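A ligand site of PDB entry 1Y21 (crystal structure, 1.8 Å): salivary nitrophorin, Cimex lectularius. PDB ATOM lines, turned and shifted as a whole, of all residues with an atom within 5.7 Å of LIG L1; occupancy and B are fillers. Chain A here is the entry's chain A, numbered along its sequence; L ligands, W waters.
The side-chain sulfur (SG) of Cys 60 lies close to a nitrogen (N2) of LIG L1 (3.5 Å).
Merely in contact with LIG L1: Ala 21, Gly 57, Gly 48, Asp 52, Thr 87, Phe 49, Asn 78, Val 44, Phe 64, Ser 16, Glu 19, Trp 14, Val 61, Arg 20, Ile 80, Pro 22, Pro 54, Gln 56 and His 18.
Hydrophobic or aromatic side chains that line LIG L1: Trp 14, Pro 22, Val 44, Phe 49, Pro 54, Val 61, Phe 64, Ile 80 and Tyr 89.
Along chain A the residues within 4 Å of LIG L1 span positions 14 to 89.
The side-chain hydroxyl (OH) of Tyr 89 lies within hydrogen-bond range of an oxygen (O2) of LIG L1, 2.6 Å away.
An oxygen (O1) of LIG L1 is in salt-bridge range of the side-chain amino group (NZ) of Lys 75 (2.7 Å).
An oxygen (O2) of LIG L1 lies within hydrogen-bond range of the side-chain amide nitrogen (NE2) of Gln 65 (2.9 Å).
A nitrogen (N1) of LG3 L3 is covalently linked to the side-chain sulfur (SG) of Cys 60.
N of Gly 57 lies within hydrogen-bond range of OD1 of Asp 52, at 2.9 Å.
N of Gln 56 sits at hydrogen-bond distance from OD2 of Asp 52 (2.9 Å).
The side-chain carboxylate (OD2) of Asp 52 lies within hydrogen-bond range of the backbone NH (N) of Gln 55.
The side-chain amide nitrogen of Asn 78 is in hydrogen-bond range of the side-chain hydroxyl of Thr 87 (2.7 Å).
The backbone carbonyl oxygen (O) of Thr 87 lies within hydrogen-bond range of the backbone NH (N) of Val 42.
The side-chain amide oxygen (OE1) of Gln 56 sits close to the guanidinium group (NH1) of Arg 20 (3.4 Å).
Water W1 lies within hydrogen-bond range of O4 of LIG L1 (2.6 Å), NZ of Lys 75 (3.0 Å) and OD1 of Asn 78 (3.3 Å).
An iron atom (FE1) of LIG L1 is bound by a nitrogen (N1) of LG2 L2 (1.9 Å).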
ATOM      1  N   TRP A  14      20.934   7.389 -21.186  1.00  0.00           N
ATOM      2  CA  TRP A  14      20.778   7.970 -19.879  1.00  0.00           C
ATOM      3  C   TRP A  14      22.084   7.917 -19.116  1.00  0.00           C
ATOM      4  O   TRP A  14      22.619   6.864 -18.872  1.00  0.00           O
ATOM      5  CB  TRP A  14      19.695   7.213 -19.147  1.00  0.00           C
ATOM      6  CG  TRP A  14      19.151   7.986 -17.990  1.00  0.00           C
ATOM      7  CD1 TRP A  14      19.447   9.282 -17.606  1.00  0.00           C
ATOM      8  CD2 TRP A  14      18.148   7.526 -17.111  1.00  0.00           C
ATOM      9  NE1 TRP A  14      18.711   9.617 -16.503  1.00  0.00           N
ATOM     10  CE2 TRP A  14      17.884   8.568 -16.183  1.00  0.00           C
ATOM     11  CE3 TRP A  14      17.420   6.327 -17.005  1.00  0.00           C
ATOM     12  CZ2 TRP A  14      16.933   8.435 -15.158  1.00  0.00           C
ATOM     13  CZ3 TRP A  14      16.475   6.205 -15.999  1.00  0.00           C
ATOM     14  CH2 TRP A  14      16.248   7.234 -15.095  1.00  0.00           C
ATOM     15  N   SER A  16      22.952   7.969 -16.109  1.00  0.00           N
ATOM     16  CA  SER A  16      22.146   7.715 -14.926  1.00  0.00           C
ATOM     17  C   SER A  16      22.918   7.599 -13.601  1.00  0.00           C
ATOM     18  O   SER A  16      22.273   7.511 -12.546  1.00  0.00           O
ATOM     19  CB  SER A  16      21.375   6.427 -15.142  1.00  0.00           C
ATOM     20  OG  SER A  16      22.278   5.455 -15.607  1.00  0.00           O
ATOM     21  N   GLY A  17      24.246   7.591 -13.635  1.00  0.00           N
ATOM     22  CA  GLY A  17      25.056   7.654 -12.412  1.00  0.00           C
ATOM     23  C   GLY A  17      24.956   6.397 -11.540  1.00  0.00           C
ATOM     24  O   GLY A  17      25.496   5.330 -11.925  1.00  0.00           O
ATOM     25  N   HIS A  18      24.282   6.532 -10.396  1.00  0.00           N
ATOM     26  CA  HIS A  18      23.977   5.428  -9.466  1.00  0.00           C
ATOM     27  C   HIS A  18      22.498   5.037  -9.476  1.00  0.00           C
ATOM     28  O   HIS A  18      22.094   4.057  -8.833  1.00  0.00           O
ATOM     29  CB  HIS A  18      24.330   5.831  -8.024  1.00  0.00           C
ATOM     30  CG  HIS A  18      25.765   6.191  -7.812  1.00  0.00           C
ATOM     31  ND1 HIS A  18      26.801   5.571  -8.478  1.00  0.00           N
ATOM     32  CD2 HIS A  18      26.328   7.121  -6.998  1.00  0.00           C
ATOM     33  CE1 HIS A  18      27.950   6.101  -8.082  1.00  0.00           C
ATOM     34  NE2 HIS A  18      27.690   7.052  -7.199  1.00  0.00           N
ATOM     35  N   GLU A  19      21.676   5.819 -10.168  1.00  0.00           N
ATOM     36  CA  GLU A  19      20.245   5.552 -10.197  1.00  0.00           C
ATOM     37  C   GLU A  19      19.937   4.205 -10.862  1.00  0.00           C
ATOM     38  O   GLU A  19      20.664   3.750 -11.762  1.00  0.00           O
ATOM     39  CB  GLU A  19      19.496   6.686 -10.895  1.00  0.00           C
ATOM     40  CG  GLU A  19      19.732   8.081 -10.280  1.00  0.00           C
ATOM     41  CD  GLU A  19      19.800   8.109  -8.734  1.00  0.00           C
ATOM     42  OE1 GLU A  19      18.746   7.847  -8.078  1.00  0.00           O
ATOM     43  OE2 GLU A  19      20.888   8.421  -8.197  1.00  0.00           O
ATOM     44  N   ARG A  20      18.852   3.585 -10.396  1.00  0.00           N
ATOM     45  CA  ARG A  20      18.486   2.222 -10.776  1.00  0.00           C
ATOM     46  C   ARG A  20      17.374   2.291 -11.826  1.00  0.00           C
ATOM     47  O   ARG A  20      16.606   3.269 -11.857  1.00  0.00           O
ATOM     48  CB  ARG A  20      18.052   1.467  -9.519  1.00  0.00           C
ATOM     49  CG  ARG A  20      18.745   1.997  -8.208  1.00  0.00           C
ATOM     50  CD  ARG A  20      18.784   1.032  -6.999  1.00  0.00           C
ATOM     51  NE  ARG A  20      18.732   1.726  -5.697  1.00  0.00           N
ATOM     52  CZ  ARG A  20      18.311   1.184  -4.533  1.00  0.00           C
ATOM     53  NH1 ARG A  20      17.882  -0.075  -4.453  1.00  0.00           N
ATOM     54  NH2 ARG A  20      18.311   1.937  -3.426  1.00  0.00           N
ATOM     55  N   ALA A  21      17.302   1.288 -12.713  1.00  0.00           N
ATOM     56  CA  ALA A  21      16.254   1.270 -13.752  1.00  0.00           C
ATOM     57  C   ALA A  21      14.914   1.640 -13.128  1.00  0.00           C
ATOM     58  O   ALA A  21      14.507   1.028 -12.141  1.00  0.00           O
ATOM     59  CB  ALA A  21      16.164  -0.080 -14.432  1.00  0.00           C
ATOM     60  N   PRO A  22      14.265   2.670 -13.645  1.00  0.00           N
ATOM     61  CA  PRO A  22      12.964   3.058 -13.095  1.00  0.00           C
ATOM     62  C   PRO A  22      11.949   1.984 -13.407  1.00  0.00           C
ATOM     63  O   PRO A  22      12.235   1.071 -14.200  1.00  0.00           O
ATOM     64  CB  PRO A  22      12.631   4.352 -13.820  1.00  0.00           C
ATOM     65  CG  PRO A  22      13.551   4.358 -15.059  1.00  0.00           C
ATOM     66  CD  PRO A  22      14.732   3.528 -14.738  1.00  0.00           C
ATOM     67  N   LEU A  28      10.397   4.973 -21.103  1.00  0.00           N
ATOM     68  CA  LEU A  28      11.833   5.074 -21.369  1.00  0.00           C
ATOM     69  C   LEU A  28      12.161   4.609 -22.810  1.00  0.00           C
ATOM     70  O   LEU A  28      12.983   5.178 -23.501  1.00  0.00           O
ATOM     71  CB  LEU A  28      12.622   4.263 -20.314  1.00  0.00           C
ATOM     72  CG  LEU A  28      14.153   4.456 -20.343  1.00  0.00           C
ATOM     73  CD1 LEU A  28      14.574   5.849 -19.896  1.00  0.00           C
ATOM     74  CD2 LEU A  28      14.873   3.399 -19.525  1.00  0.00           C
ATOM     75  N   VAL A  42      19.647   0.595 -25.806  1.00  0.00           N
ATOM     76  CA  VAL A  42      19.722   1.281 -24.523  1.00  0.00           C
ATOM     77  C   VAL A  42      21.184   1.465 -24.098  1.00  0.00           C
ATOM     78  O   VAL A  42      21.946   0.507 -23.859  1.00  0.00           O
ATOM     79  CB  VAL A  42      18.913   0.511 -23.421  1.00  0.00           C
ATOM     80  CG1 VAL A  42      18.908   1.299 -22.160  1.00  0.00           C
ATOM     81  CG2 VAL A  42      17.444   0.236 -23.956  1.00  0.00           C
ATOM     82  N   VAL A  44      23.696   3.409 -21.199  1.00  0.00           N
ATOM     83  CA  VAL A  44      23.787   4.084 -19.919  1.00  0.00           C
ATOM     84  C   VAL A  44      25.222   4.405 -19.593  1.00  0.00           C
ATOM     85  O   VAL A  44      26.181   3.736 -20.033  1.00  0.00           O
ATOM     86  CB  VAL A  44      23.082   3.281 -18.777  1.00  0.00           C
ATOM     87  CG1 VAL A  44      21.686   3.070 -19.112  1.00  0.00           C
ATOM     88  CG2 VAL A  44      23.746   1.938 -18.540  1.00  0.00           C
ATOM     89  N   PHE A  47      28.749   4.638 -12.813  1.00  0.00           N
ATOM     90  CA  PHE A  47      29.909   4.309 -11.963  1.00  0.00           C
ATOM     91  C   PHE A  47      29.628   2.931 -11.346  1.00  0.00           C
ATOM     92  O   PHE A  47      28.539   2.700 -10.844  1.00  0.00           O
ATOM     93  CB  PHE A  47      30.058   5.337 -10.813  1.00  0.00           C
ATOM     94  CG  PHE A  47      30.102   6.798 -11.250  1.00  0.00           C
ATOM     95  CD1 PHE A  47      28.998   7.638 -11.050  1.00  0.00           C
ATOM     96  CD2 PHE A  47      31.263   7.339 -11.834  1.00  0.00           C
ATOM     97  CE1 PHE A  47      29.034   9.010 -11.444  1.00  0.00           C
ATOM     98  CE2 PHE A  47      31.317   8.721 -12.240  1.00  0.00           C
ATOM     99  CZ  PHE A  47      30.200   9.543 -12.038  1.00  0.00           C
ATOM    100  N   GLY A  48      30.594   2.013 -11.446  1.00  0.00           N
ATOM    101  CA  GLY A  48      30.486   0.680 -10.870  1.00  0.00           C
ATOM    102  C   GLY A  48      29.441  -0.331 -11.364  1.00  0.00           C
ATOM    103  O   GLY A  48      29.001  -1.181 -10.574  1.00  0.00           O
ATOM    104  N   PHE A  49      29.063  -0.310 -12.647  1.00  0.00           N
ATOM    105  CA  PHE A  49      28.117  -1.316 -13.165  1.00  0.00           C
ATOM    106  C   PHE A  49      28.644  -2.744 -13.041  1.00  0.00           C
ATOM    107  O   PHE A  49      27.914  -3.640 -12.622  1.00  0.00           O
ATOM    108  CB  PHE A  49      27.793  -1.108 -14.655  1.00  0.00           C
ATOM    109  CG  PHE A  49      27.153   0.210 -14.963  1.00  0.00           C
ATOM    110  CD1 PHE A  49      27.645   1.001 -15.977  1.00  0.00           C
ATOM    111  CD2 PHE A  49      26.060   0.652 -14.248  1.00  0.00           C
ATOM    112  CE1 PHE A  49      27.035   2.202 -16.268  1.00  0.00           C
ATOM    113  CE2 PHE A  49      25.449   1.884 -14.517  1.00  0.00           C
ATOM    114  CZ  PHE A  49      25.942   2.678 -15.544  1.00  0.00           C
ATOM    115  N   GLN A  50      29.905  -2.921 -13.432  1.00  0.00           N
ATOM    116  CA  GLN A  50      30.574  -4.208 -13.450  1.00  0.00           C
ATOM    117  C   GLN A  50      30.729  -4.844 -12.077  1.00  0.00           C
ATOM    118  O   GLN A  50      30.317  -5.980 -11.872  1.00  0.00           O
ATOM    119  CB  GLN A  50      31.941  -4.060 -14.100  1.00  0.00           C
ATOM    120  CG  GLN A  50      32.266  -5.185 -15.053  1.00  0.00           C
ATOM    121  CD  GLN A  50      33.578  -4.988 -15.737  1.00  0.00           C
ATOM    122  OE1 GLN A  50      34.013  -5.825 -16.550  1.00  0.00           O
ATOM    123  NE2 GLN A  50      34.410  -3.951 -15.587  1.00  0.00           N
ATOM    124  N   ASP A  52      28.944  -4.136  -9.757  1.00  0.00           N
ATOM    125  CA  ASP A  52      27.499  -4.295  -9.352  1.00  0.00           C
ATOM    126  C   ASP A  52      27.360  -4.504  -7.828  1.00  0.00           C
ATOM    127  O   ASP A  52      26.883  -5.541  -7.340  1.00  0.00           O
ATOM    128  CB  ASP A  52      26.828  -5.446 -10.085  1.00  0.00           C
ATOM    129  CG  ASP A  52      25.337  -5.413  -9.832  1.00  0.00           C
ATOM    130  OD1 ASP A  52      24.659  -6.404 -10.170  1.00  0.00           O
ATOM    131  OD2 ASP A  52      24.854  -4.395  -9.319  1.00  0.00           O
ATOM    132  N   LYS A  53      27.780  -3.455  -7.063  1.00  0.00           N
ATOM    133  CA  LYS A  53      27.763  -3.460  -5.595  1.00  0.00           C
ATOM    134  C   LYS A  53      26.337  -3.256  -5.022  1.00  0.00           C
ATOM    135  O   LYS A  53      26.042  -3.874  -3.988  1.00  0.00           O
ATOM    136  CB  LYS A  53      28.739  -2.426  -4.996  1.00  0.00           C
ATOM    137  CG  LYS A  53      29.133  -2.703  -3.542  1.00  0.00           C
ATOM    138  CD  LYS A  53      30.401  -1.980  -3.088  1.00  0.00           C
ATOM    139  CE  LYS A  53      30.774  -2.400  -1.676  1.00  0.00           C
ATOM    140  NZ  LYS A  53      32.014  -3.229  -1.658  1.00  0.00           N
ATOM    141  N   PRO A  54      25.448  -2.411  -5.628  1.00  0.00           N
ATOM    142  CA  PRO A  54      24.052  -2.389  -5.163  1.00  0.00           C
ATOM    143  C   PRO A  54      23.262  -3.634  -5.653  1.00  0.00           C
ATOM    144  O   PRO A  54      22.114  -3.825  -5.239  1.00  0.00           O
ATOM    145  CB  PRO A  54      23.474  -1.081  -5.770  1.00  0.00           C
ATOM    146  CG  PRO A  54      24.615  -0.378  -6.432  1.00  0.00           C
ATOM    147  CD  PRO A  54      25.654  -1.435  -6.716  1.00  0.00           C
ATOM    148  N   GLN A  55      23.844  -4.497  -6.511  1.00  0.00           N
ATOM    149  CA  GLN A  55      23.140  -5.704  -7.012  1.00  0.00           C
ATOM    150  C   GLN A  55      21.886  -5.387  -7.861  1.00  0.00           C
ATOM    151  O   GLN A  55      20.857  -6.053  -7.746  1.00  0.00           O
ATOM    152  CB  GLN A  55      22.793  -6.617  -5.840  1.00  0.00           C
ATOM    153  CG  GLN A  55      24.010  -7.266  -5.189  1.00  0.00           C
ATOM    154  CD  GLN A  55      23.628  -7.906  -3.866  1.00  0.00           C
ATOM    155  OE1 GLN A  55      23.331  -9.092  -3.822  1.00  0.00           O
ATOM    156  NE2 GLN A  55      23.575  -7.314  -2.683  1.00  0.00           N
ATOM    157  N   GLN A  56      21.998  -4.350  -8.683  1.00  0.00           N
ATOM    158  CA  GLN A  56      20.922  -3.907  -9.590  1.00  0.00           C
ATOM    159  C   GLN A  56      20.947  -4.766 -10.875  1.00  0.00           C
ATOM    160  O   GLN A  56      19.970  -4.813 -11.598  1.00  0.00           O
ATOM    161  CB  GLN A  56      21.049  -2.432  -9.941  1.00  0.00           C
ATOM    162  CG  GLN A  56      20.633  -1.402  -8.891  1.00  0.00           C
ATOM    163  CD  GLN A  56      19.408  -1.816  -8.075  1.00  0.00           C
ATOM    164  OE1 GLN A  56      19.453  -1.829  -6.846  1.00  0.00           O
ATOM    165  NE2 GLN A  56      18.219  -2.194  -8.559  1.00  0.00           N
ATOM    166  N   GLY A  57      22.076  -5.439 -11.128  1.00  0.00           N
ATOM    167  CA  GLY A  57      22.230  -6.317 -12.260  1.00  0.00           C
ATOM    168  C   GLY A  57      21.086  -7.299 -12.459  1.00  0.00           C
ATOM    169  O   GLY A  57      20.389  -7.225 -13.464  1.00  0.00           O
ATOM    170  N   PRO A  58      20.897  -8.237 -11.529  1.00  0.00           N
ATOM    171  CA  PRO A  58      19.792  -9.180 -11.644  1.00  0.00           C
ATOM    172  C   PRO A  58      18.450  -8.480 -11.843  1.00  0.00           C
ATOM    173  O   PRO A  58      17.721  -8.936 -12.694  1.00  0.00           O
ATOM    174  CB  PRO A  58      19.840  -9.964 -10.296  1.00  0.00           C
ATOM    175  CG  PRO A  58      21.290  -9.900  -9.894  1.00  0.00           C
ATOM    176  CD  PRO A  58      21.757  -8.531 -10.353  1.00  0.00           C
ATOM    177  N   CYS A  60      17.779  -5.553 -13.269  1.00  0.00           N
ATOM    178  CA  CYS A  60      17.797  -5.006 -14.621  1.00  0.00           C
ATOM    179  C   CYS A  60      17.352  -6.052 -15.590  1.00  0.00           C
ATOM    180  O   CYS A  60      16.430  -5.794 -16.398  1.00  0.00           O
ATOM    181  CB  CYS A  60      19.178  -4.526 -15.074  1.00  0.00           C
ATOM    182  SG  CYS A  60      19.678  -3.040 -14.251  1.00  0.00           S
ATOM    183  N   VAL A  61      17.965  -7.225 -15.517  1.00  0.00           N
ATOM    184  CA  VAL A  61      17.716  -8.291 -16.483  1.00  0.00           C
ATOM    185  C   VAL A  61      16.250  -8.686 -16.377  1.00  0.00           C
ATOM    186  O   VAL A  61      15.531  -8.716 -17.371  1.00  0.00           O
ATOM    187  CB  VAL A  61      18.588  -9.563 -16.243  1.00  0.00           C
ATOM    188  CG1 VAL A  61      18.193 -10.635 -17.260  1.00  0.00           C
ATOM    189  CG2 VAL A  61      20.123  -9.277 -16.366  1.00  0.00           C
ATOM    190  N   PHE A  64      13.776  -5.784 -17.656  1.00  0.00           N
ATOM    191  CA  PHE A  64      13.859  -5.615 -19.111  1.00  0.00           C
ATOM    192  C   PHE A  64      13.395  -6.874 -19.841  1.00  0.00           C
ATOM    193  O   PHE A  64      12.594  -6.769 -20.776  1.00  0.00           O
ATOM    194  CB  PHE A  64      15.267  -5.202 -19.558  1.00  0.00           C
ATOM    195  CG  PHE A  64      15.467  -3.729 -19.535  1.00  0.00           C
ATOM    196  CD1 PHE A  64      16.079  -3.114 -18.454  1.00  0.00           C
ATOM    197  CD2 PHE A  64      15.001  -2.945 -20.607  1.00  0.00           C
ATOM    198  CE1 PHE A  64      16.229  -1.714 -18.423  1.00  0.00           C
ATOM    199  CE2 PHE A  64      15.159  -1.568 -20.581  1.00  0.00           C
ATOM    200  CZ  PHE A  64      15.788  -0.944 -19.511  1.00  0.00           C
ATOM    201  N   GLN A  65      13.861  -8.049 -19.388  1.00  0.00           N
ATOM    202  CA  GLN A  65      13.539  -9.310 -20.062  1.00  0.00           C
ATOM    203  C   GLN A  65      12.071  -9.625 -20.017  1.00  0.00           C
ATOM    204  O   GLN A  65      11.492 -10.014 -21.028  1.00  0.00           O
ATOM    205  CB  GLN A  65      14.316 -10.543 -19.547  1.00  0.00           C
ATOM    206  CG  GLN A  65      15.840 -10.480 -19.775  1.00  0.00           C
ATOM    207  CD  GLN A  65      16.305 -10.962 -21.128  1.00  0.00           C
ATOM    208  OE1 GLN A  65      16.651 -12.142 -21.263  1.00  0.00           O
ATOM    209  NE2 GLN A  65      16.401 -10.042 -22.102  1.00  0.00           N
ATOM    210  N   LYS A  75      17.105 -10.265 -26.878  1.00  0.00           N
ATOM    211  CA  LYS A  75      18.303  -9.477 -26.542  1.00  0.00           C
ATOM    212  C   LYS A  75      19.520  -9.994 -27.315  1.00  0.00           C
ATOM    213  O   LYS A  75      19.942 -11.133 -27.110  1.00  0.00           O
ATOM    214  CB  LYS A  75      18.604  -9.590 -25.073  1.00  0.00           C
ATOM    215  CG  LYS A  75      19.991  -9.004 -24.670  1.00  0.00           C
ATOM    216  CD  LYS A  75      20.166  -9.035 -23.193  1.00  0.00           C
ATOM    217  CE  LYS A  75      20.634 -10.361 -22.755  1.00  0.00           C
ATOM    218  NZ  LYS A  75      20.560 -10.414 -21.286  1.00  0.00           N
ATOM    219  N   ASN A  78      24.044  -7.628 -24.248  1.00  0.00           N
ATOM    220  CA  ASN A  78      24.212  -6.662 -23.186  1.00  0.00           C
ATOM    221  C   ASN A  78      25.706  -6.650 -22.910  1.00  0.00           C
ATOM    222  O   ASN A  78      26.365  -7.726 -22.820  1.00  0.00           O
ATOM    223  CB  ASN A  78      23.407  -6.997 -21.942  1.00  0.00           C
ATOM    224  CG  ASN A  78      23.829  -6.170 -20.728  1.00  0.00           C
ATOM    225  OD1 ASN A  78      24.472  -6.681 -19.854  1.00  0.00           O
ATOM    226  ND2 ASN A  78      23.467  -4.871 -20.689  1.00  0.00           N
ATOM    227  N   ILE A  80      28.549  -4.519 -20.347  1.00  0.00           N
ATOM    228  CA  ILE A  80      28.789  -3.561 -19.255  1.00  0.00           C
ATOM    229  C   ILE A  80      30.298  -3.420 -18.999  1.00  0.00           C
ATOM    230  O   ILE A  80      31.061  -4.406 -19.057  1.00  0.00           O
ATOM    231  CB  ILE A  80      28.067  -3.995 -17.966  1.00  0.00           C
ATOM    232  CG1 ILE A  80      28.294  -5.480 -17.677  1.00  0.00           C
ATOM    233  CG2 ILE A  80      26.588  -3.766 -18.110  1.00  0.00           C
ATOM    234  CD1 ILE A  80      28.293  -5.890 -16.182  1.00  0.00           C
ATOM    235  N   THR A  87      22.891  -2.190 -24.435  1.00  0.00           N
ATOM    236  CA  THR A  87      22.025  -3.352 -24.726  1.00  0.00           C
ATOM    237  C   THR A  87      21.340  -3.118 -26.026  1.00  0.00           C
ATOM    238  O   THR A  87      20.756  -2.031 -26.264  1.00  0.00           O
ATOM    239  CB  THR A  87      21.005  -3.517 -23.594  1.00  0.00           C
ATOM    240  OG1 THR A  87      21.702  -3.569 -22.337  1.00  0.00           O
ATOM    241  CG2 THR A  87      20.245  -4.883 -23.683  1.00  0.00           C
ATOM    242  N   TYR A  89      18.359  -4.915 -28.622  1.00  0.00           N
ATOM    243  CA  TYR A  89      17.240  -5.860 -28.826  1.00  0.00           C
ATOM    244  C   TYR A  89      16.732  -5.802 -30.258  1.00  0.00           C
ATOM    245  O   TYR A  89      16.650  -4.751 -30.865  1.00  0.00           O
ATOM    246  CB  TYR A  89      16.070  -5.460 -27.913  1.00  0.00           C
ATOM    247  CG  TYR A  89      16.351  -5.431 -26.418  1.00  0.00           C
ATOM    248  CD1 TYR A  89      16.719  -4.242 -25.766  1.00  0.00           C
ATOM    249  CD2 TYR A  89      16.252  -6.561 -25.654  1.00  0.00           C
ATOM    250  CE1 TYR A  89      16.980  -4.237 -24.394  1.00  0.00           C
ATOM    251  CE2 TYR A  89      16.480  -6.546 -24.295  1.00  0.00           C
ATOM    252  CZ  TYR A  89      16.873  -5.371 -23.661  1.00  0.00           C
ATOM    253  OH  TYR A  89      17.128  -5.259 -22.336  1.00  0.00           O
HETATM  254  C1  LIG L   1      22.076  -5.121 -17.290  1.00  0.00           C
HETATM  255  C2  LIG L   1      19.854  -0.942 -18.323  1.00  0.00           C
HETATM  256  C3  LIG L   1      21.546   0.774 -14.104  1.00  0.00           C
HETATM  257  C4  LIG L   1      24.431  -3.116 -13.487  1.00  0.00           C
HETATM  258  C5  LIG L   1      21.302  -4.197 -17.902  1.00  0.00           C
HETATM  259  C6  LIG L   1      20.444  -4.397 -19.052  1.00  0.00           C
HETATM  260  C7  LIG L   1      19.846  -3.214 -19.340  1.00  0.00           C
HETATM  261  C8  LIG L   1      20.273  -2.264 -18.366  1.00  0.00           C
HETATM  262  C9  LIG L   1      18.884  -2.856 -20.511  1.00  0.00           C
HETATM  263  C10 LIG L   1      20.250  -5.717 -19.830  1.00  0.00           C
HETATM  264  C11 LIG L   1      18.785  -6.128 -19.633  1.00  0.00           C
HETATM  265  C12 LIG L   1      18.551  -7.475 -20.296  1.00  0.00           C
HETATM  266  O1  LIG L   1      19.374  -8.401 -19.945  1.00  0.00           O
HETATM  267  O2  LIG L   1      17.640  -7.556 -21.178  1.00  0.00           O
HETATM  268  C13 LIG L   1      20.060  -0.099 -17.245  1.00  0.00           C
HETATM  269  C14 LIG L   1      19.526   1.246 -17.076  1.00  0.00           C
HETATM  270  C15 LIG L   1      20.015   1.702 -15.900  1.00  0.00           C
HETATM  271  C16 LIG L   1      20.854   0.696 -15.291  1.00  0.00           C
HETATM  272  C17 LIG L   1      18.579   1.943 -18.077  1.00  0.00           C
HETATM  273  C18 LIG L   1      19.743   3.066 -15.251  1.00  0.00           C
HETATM  274  C19 LIG L   1      18.463   3.464 -15.063  1.00  0.00           C
HETATM  275  C20 LIG L   1      22.450  -0.120 -13.589  1.00  0.00           C
HETATM  276  C21 LIG L   1      23.161   0.022 -12.321  1.00  0.00           C
HETATM  277  C22 LIG L   1      23.936  -1.059 -12.162  1.00  0.00           C
HETATM  278  C23 LIG L   1      23.764  -1.928 -13.303  1.00  0.00           C
HETATM  279  C24 LIG L   1      23.052   1.217 -11.321  1.00  0.00           C
HETATM  280  C25 LIG L   1      24.911  -1.399 -10.993  1.00  0.00           C
HETATM  281  C26 LIG L   1      25.657  -0.448 -10.393  1.00  0.00           C
HETATM  282  C27 LIG L   1      24.055  -4.056 -14.405  1.00  0.00           C
HETATM  283  C28 LIG L   1      24.547  -5.396 -14.545  1.00  0.00           C
HETATM  284  C29 LIG L   1      23.812  -5.987 -15.749  1.00  0.00           C
HETATM  285  C30 LIG L   1      22.946  -4.940 -16.232  1.00  0.00           C
HETATM  286  C31 LIG L   1      25.589  -6.140 -13.698  1.00  0.00           C
HETATM  287  C32 LIG L   1      23.946  -7.426 -16.311  1.00  0.00           C
HETATM  288  C33 LIG L   1      23.472  -8.483 -15.325  1.00  0.00           C
HETATM  289  C34 LIG L   1      23.563  -9.867 -15.941  1.00  0.00           C
HETATM  290  O3  LIG L   1      23.549 -10.861 -15.149  1.00  0.00           O
HETATM  291  O4  LIG L   1      23.669  -9.946 -17.209  1.00  0.00           O
HETATM  292  N1  LIG L   1      21.173  -2.880 -17.500  1.00  0.00           N
HETATM  293  N2  LIG L   1      20.855  -0.361 -16.173  1.00  0.00           N
HETATM  294  N3  LIG L   1      22.848  -1.320 -14.157  1.00  0.00           N
HETATM  295  N4  LIG L   1      23.152  -3.820 -15.415  1.00  0.00           N
HETATM  296 FE1  LIG L   1      22.086  -1.999 -15.929  1.00  0.00          FE
HETATM  297  N1  LG2 L   2      23.510  -1.262 -16.856  1.00  0.00           N
HETATM  298  O1  LG2 L   2      23.542  -1.361 -18.212  1.00  0.00           O
HETATM  299  N1  LG3 L   3      18.699  -1.844 -14.980  1.00  0.00           N
HETATM  300  O1  LG3 L   3      17.908  -2.134 -15.879  1.00  0.00           O
HETATM  301  O   HOH W   1      22.267  -9.043 -19.195  1.00  0.00           O
